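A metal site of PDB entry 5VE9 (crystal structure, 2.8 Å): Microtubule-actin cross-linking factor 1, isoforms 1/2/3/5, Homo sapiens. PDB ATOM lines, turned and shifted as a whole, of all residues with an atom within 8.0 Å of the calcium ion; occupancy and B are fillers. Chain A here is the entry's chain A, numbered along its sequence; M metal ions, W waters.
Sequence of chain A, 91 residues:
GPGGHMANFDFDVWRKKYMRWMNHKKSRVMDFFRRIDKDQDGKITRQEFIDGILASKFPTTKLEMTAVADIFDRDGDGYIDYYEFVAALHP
OD1 of Asp 73 sits close to N of Gly 76, 3.4 Å away.
The side-chain carboxylate (OD2) of Asp 73 sits at hydrogen-bond distance from the backbone NH (N) of Gly 78, at 2.9 Å.
OD2 of Asp 73 lies within salt-bridge range of NH2 of Arg 46 (2.9 Å).
The side-chain carboxylate of Asp 81 sits at hydrogen-bond distance from the backbone NH of Glu 84 (2.8 Å).
OE2 of Glu 84 lies close to N of Arg 74, at 3.5 Å.
The calcium ion is bound by the backbone carbonyl oxygen (O) of Tyr 79 (2.2 Å), the side-chain carboxylate (OD1) of Asp 75 (2.3 Å), the side-chain carboxylate (OD1) of Asp 73 (2.4 Å), the side-chain carboxylate (OE1) of Glu 84 (2.4 Å), water W1 (2.5 Å), the side-chain carboxylate (OD2) of Asp 77 (2.5 Å), the side-chain carboxylate (OE2) of Glu 84 (2.5 Å) and the side-chain carboxylate (OD2) of Asp 75 (2.7 Å).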
ATOM      1  N   LYS A  43      11.541  16.059   0.037  1.00  0.00           N
ATOM      2  CA  LYS A  43      12.419  15.694   1.154  1.00  0.00           C
ATOM      3  C   LYS A  43      13.569  14.814   0.683  1.00  0.00           C
ATOM      4  O   LYS A  43      13.442  14.071  -0.292  1.00  0.00           O
ATOM      5  CB  LYS A  43      11.627  14.965   2.245  1.00  0.00           C
ATOM      6  CG  LYS A  43      10.450  15.747   2.812  1.00  0.00           C
ATOM      7  CD  LYS A  43       9.446  14.828   3.510  1.00  0.00           C
ATOM      8  CE  LYS A  43       9.983  14.272   4.825  1.00  0.00           C
ATOM      9  NZ  LYS A  43       9.161  13.130   5.328  1.00  0.00           N
ATOM     10  N   ILE A  44      14.696  14.916   1.374  1.00  0.00           N
ATOM     11  CA  ILE A  44      15.808  13.987   1.197  1.00  0.00           C
ATOM     12  C   ILE A  44      16.449  13.747   2.554  1.00  0.00           C
ATOM     13  O   ILE A  44      16.610  14.688   3.349  1.00  0.00           O
ATOM     14  CB  ILE A  44      16.868  14.502   0.192  1.00  0.00           C
ATOM     15  CG1 ILE A  44      17.392  15.878   0.604  1.00  0.00           C
ATOM     16  CG2 ILE A  44      16.263  14.555  -1.220  1.00  0.00           C
ATOM     17  CD1 ILE A  44      18.452  16.435  -0.324  1.00  0.00           C
ATOM     18  N   ARG A  46      19.285  13.045   5.406  1.00  0.00           N
ATOM     19  CA  ARG A  46      20.632  13.564   5.614  1.00  0.00           C
ATOM     20  C   ARG A  46      21.642  12.745   4.816  1.00  0.00           C
ATOM     21  O   ARG A  46      22.590  13.292   4.254  1.00  0.00           O
ATOM     22  CB  ARG A  46      21.016  13.535   7.095  1.00  0.00           C
ATOM     23  CG  ARG A  46      20.157  14.413   7.995  1.00  0.00           C
ATOM     24  CD  ARG A  46      20.803  14.534   9.366  1.00  0.00           C
ATOM     25  NE  ARG A  46      19.890  15.067  10.378  1.00  0.00           N
ATOM     26  CZ  ARG A  46      20.281  15.539  11.559  1.00  0.00           C
ATOM     27  NH1 ARG A  46      21.571  15.553  11.879  1.00  0.00           N
ATOM     28  NH2 ARG A  46      19.381  15.995  12.428  1.00  0.00           N
ATOM     29  N   ALA A  69      25.153  18.614   6.913  1.00  0.00           N
ATOM     30  CA  ALA A  69      23.849  17.955   6.845  1.00  0.00           C
ATOM     31  C   ALA A  69      23.091  18.174   8.152  1.00  0.00           C
ATOM     32  O   ALA A  69      21.864  18.224   8.165  1.00  0.00           O
ATOM     33  CB  ALA A  69      24.012  16.458   6.568  1.00  0.00           C
ATOM     34  N   PHE A  72      21.803  21.865   7.800  1.00  0.00           N
ATOM     35  CA  PHE A  72      20.678  21.902   6.870  1.00  0.00           C
ATOM     36  C   PHE A  72      19.394  21.455   7.525  1.00  0.00           C
ATOM     37  O   PHE A  72      18.360  22.116   7.427  1.00  0.00           O
ATOM     38  CB  PHE A  72      20.963  21.033   5.650  1.00  0.00           C
ATOM     39  CG  PHE A  72      21.633  21.753   4.512  1.00  0.00           C
ATOM     40  CD1 PHE A  72      22.917  22.251   4.667  1.00  0.00           C
ATOM     41  CD2 PHE A  72      20.983  21.937   3.306  1.00  0.00           C
ATOM     42  CE1 PHE A  72      23.539  22.919   3.632  1.00  0.00           C
ATOM     43  CE2 PHE A  72      21.603  22.596   2.269  1.00  0.00           C
ATOM     44  CZ  PHE A  72      22.878  23.093   2.434  1.00  0.00           C
ATOM     45  N   ASP A  73      19.443  20.308   8.198  1.00  0.00           N
ATOM     46  CA  ASP A  73      18.267  19.772   8.878  1.00  0.00           C
ATOM     47  C   ASP A  73      17.917  20.625  10.098  1.00  0.00           C
ATOM     48  O   ASP A  73      18.208  20.251  11.239  1.00  0.00           O
ATOM     49  CB  ASP A  73      18.504  18.321   9.298  1.00  0.00           C
ATOM     50  CG  ASP A  73      17.235  17.636   9.767  1.00  0.00           C
ATOM     51  OD1 ASP A  73      16.146  18.103   9.367  1.00  0.00           O
ATOM     52  OD2 ASP A  73      17.316  16.639  10.519  1.00  0.00           O
ATOM     53  N   ARG A  74      17.279  21.759   9.850  1.00  0.00           N
ATOM     54  CA  ARG A  74      17.068  22.760  10.896  1.00  0.00           C
ATOM     55  C   ARG A  74      16.076  22.323  11.974  1.00  0.00           C
ATOM     56  O   ARG A  74      16.127  22.847  13.094  1.00  0.00           O
ATOM     57  CB  ARG A  74      16.603  24.068  10.258  1.00  0.00           C
ATOM     58  CG  ARG A  74      16.643  25.263  11.199  1.00  0.00           C
ATOM     59  CD  ARG A  74      16.664  26.578  10.418  1.00  0.00           C
ATOM     60  NE  ARG A  74      16.771  27.745  11.292  1.00  0.00           N
ATOM     61  CZ  ARG A  74      17.044  28.973  10.862  1.00  0.00           C
ATOM     62  NH1 ARG A  74      17.238  29.205   9.570  1.00  0.00           N
ATOM     63  NH2 ARG A  74      17.117  29.976  11.737  1.00  0.00           N
ATOM     64  N   ASP A  75      15.183  21.390  11.654  1.00  0.00           N
ATOM     65  CA  ASP A  75      14.222  20.882  12.622  1.00  0.00           C
ATOM     66  C   ASP A  75      14.757  19.646  13.352  1.00  0.00           C
ATOM     67  O   ASP A  75      14.373  19.361  14.484  1.00  0.00           O
ATOM     68  CB  ASP A  75      12.876  20.561  11.950  1.00  0.00           C
ATOM     69  CG  ASP A  75      13.000  19.524  10.847  1.00  0.00           C
ATOM     70  OD1 ASP A  75      14.057  18.879  10.737  1.00  0.00           O
ATOM     71  OD2 ASP A  75      12.022  19.354  10.079  1.00  0.00           O
ATOM     72  N   GLY A  76      15.624  18.905  12.666  1.00  0.00           N
ATOM     73  CA  GLY A  76      16.242  17.726  13.250  1.00  0.00           C
ATOM     74  C   GLY A  76      15.420  16.460  13.109  1.00  0.00           C
ATOM     75  O   GLY A  76      15.663  15.480  13.811  1.00  0.00           O
ATOM     76  N   ASP A  77      14.439  16.474  12.202  1.00  0.00           N
ATOM     77  CA  ASP A  77      13.569  15.313  12.006  1.00  0.00           C
ATOM     78  C   ASP A  77      14.226  14.239  11.141  1.00  0.00           C
ATOM     79  O   ASP A  77      13.595  13.248  10.791  1.00  0.00           O
ATOM     80  CB  ASP A  77      12.240  15.742  11.369  1.00  0.00           C
ATOM     81  CG  ASP A  77      12.396  16.203   9.924  1.00  0.00           C
ATOM     82  OD1 ASP A  77      11.387  16.202   9.194  1.00  0.00           O
ATOM     83  OD2 ASP A  77      13.521  16.550   9.513  1.00  0.00           O
ATOM     84  N   GLY A  78      15.498  14.454  10.791  1.00  0.00           N
ATOM     85  CA  GLY A  78      16.230  13.492   9.990  1.00  0.00           C
ATOM     86  C   GLY A  78      16.154  13.771   8.493  1.00  0.00           C
ATOM     87  O   GLY A  78      17.000  13.271   7.740  1.00  0.00           O
ATOM     88  N   TYR A  79      15.157  14.544   8.070  1.00  0.00           N
ATOM     89  CA  TYR A  79      14.978  14.868   6.649  1.00  0.00           C
ATOM     90  C   TYR A  79      15.305  16.314   6.340  1.00  0.00           C
ATOM     91  O   TYR A  79      14.924  17.212   7.092  1.00  0.00           O
ATOM     92  CB  TYR A  79      13.537  14.602   6.226  1.00  0.00           C
ATOM     93  CG  TYR A  79      13.198  13.146   6.057  1.00  0.00           C
ATOM     94  CD1 TYR A  79      13.503  12.484   4.883  1.00  0.00           C
ATOM     95  CD2 TYR A  79      12.556  12.446   7.072  1.00  0.00           C
ATOM     96  CE1 TYR A  79      13.180  11.151   4.722  1.00  0.00           C
ATOM     97  CE2 TYR A  79      12.226  11.124   6.915  1.00  0.00           C
ATOM     98  CZ  TYR A  79      12.553  10.479   5.735  1.00  0.00           C
ATOM     99  OH  TYR A  79      12.232   9.143   5.583  1.00  0.00           O
ATOM    100  N   ILE A  80      15.988  16.541   5.218  1.00  0.00           N
ATOM    101  CA  ILE A  80      16.183  17.899   4.711  1.00  0.00           C
ATOM    102  C   ILE A  80      15.109  18.203   3.675  1.00  0.00           C
ATOM    103  O   ILE A  80      15.135  17.645   2.568  1.00  0.00           O
ATOM    104  CB  ILE A  80      17.586  18.084   4.107  1.00  0.00           C
ATOM    105  CG1 ILE A  80      18.648  17.603   5.097  1.00  0.00           C
ATOM    106  CG2 ILE A  80      17.812  19.545   3.727  1.00  0.00           C
ATOM    107  CD1 ILE A  80      20.062  17.685   4.574  1.00  0.00           C
ATOM    108  N   ASP A  81      14.166  19.082   4.012  1.00  0.00           N
ATOM    109  CA  ASP A  81      13.088  19.400   3.075  1.00  0.00           C
ATOM    110  C   ASP A  81      13.484  20.593   2.201  1.00  0.00           C
ATOM    111  O   ASP A  81      14.559  21.173   2.368  1.00  0.00           O
ATOM    112  CB  ASP A  81      11.763  19.678   3.826  1.00  0.00           C
ATOM    113  CG  ASP A  81      11.812  20.912   4.705  1.00  0.00           C
ATOM    114  OD1 ASP A  81      12.120  22.014   4.200  1.00  0.00           O
ATOM    115  OD2 ASP A  81      11.534  20.778   5.920  1.00  0.00           O
ATOM    116  N   TYR A  82      12.608  20.934   1.266  1.00  0.00           N
ATOM    117  CA  TYR A  82      12.873  21.977   0.290  1.00  0.00           C
ATOM    118  C   TYR A  82      13.160  23.331   0.936  1.00  0.00           C
ATOM    119  O   TYR A  82      14.074  24.056   0.520  1.00  0.00           O
ATOM    120  CB  TYR A  82      11.693  22.111  -0.667  1.00  0.00           C
ATOM    121  CG  TYR A  82      12.078  22.424  -2.096  1.00  0.00           C
ATOM    122  CD1 TYR A  82      12.783  21.497  -2.851  1.00  0.00           C
ATOM    123  CD2 TYR A  82      11.723  23.623  -2.684  1.00  0.00           C
ATOM    124  CE1 TYR A  82      13.128  21.770  -4.153  1.00  0.00           C
ATOM    125  CE2 TYR A  82      12.060  23.910  -3.990  1.00  0.00           C
ATOM    126  CZ  TYR A  82      12.767  22.974  -4.717  1.00  0.00           C
ATOM    127  OH  TYR A  82      13.122  23.245  -6.020  1.00  0.00           O
ATOM    128  N   GLU A  84      14.092  24.017   4.108  1.00  0.00           N
ATOM    129  CA  GLU A  84      15.341  23.960   4.864  1.00  0.00           C
ATOM    130  C   GLU A  84      16.524  24.120   3.931  1.00  0.00           C
ATOM    131  O   GLU A  84      17.464  24.859   4.215  1.00  0.00           O
ATOM    132  CB  GLU A  84      15.434  22.652   5.638  1.00  0.00           C
ATOM    133  CG  GLU A  84      14.534  22.616   6.841  1.00  0.00           C
ATOM    134  CD  GLU A  84      14.592  21.277   7.566  1.00  0.00           C
ATOM    135  OE1 GLU A  84      15.189  20.327   7.012  1.00  0.00           O
ATOM    136  OE2 GLU A  84      14.039  21.181   8.679  1.00  0.00           O
ATOM    137  N   PHE A  85      16.473  23.403   2.811  1.00  0.00           N
ATOM    138  CA  PHE A  85      17.490  23.487   1.772  1.00  0.00           C
ATOM    139  C   PHE A  85      17.724  24.935   1.323  1.00  0.00           C
ATOM    140  O   PHE A  85      18.833  25.450   1.392  1.00  0.00           O
ATOM    141  CB  PHE A  85      17.096  22.612   0.575  1.00  0.00           C
ATOM    142  CG  PHE A  85      18.187  22.445  -0.447  1.00  0.00           C
ATOM    143  CD1 PHE A  85      19.202  21.520  -0.246  1.00  0.00           C
ATOM    144  CD2 PHE A  85      18.197  23.193  -1.617  1.00  0.00           C
ATOM    145  CE1 PHE A  85      20.205  21.358  -1.174  1.00  0.00           C
ATOM    146  CE2 PHE A  85      19.197  23.025  -2.558  1.00  0.00           C
ATOM    147  CZ  PHE A  85      20.205  22.108  -2.342  1.00  0.00           C
HETATM  148 CA    CA M   1      14.042  18.707   8.420  1.00  0.00          CA
HETATM  149  O   HOH W   1      11.918  18.917   7.196  1.00  0.00           O
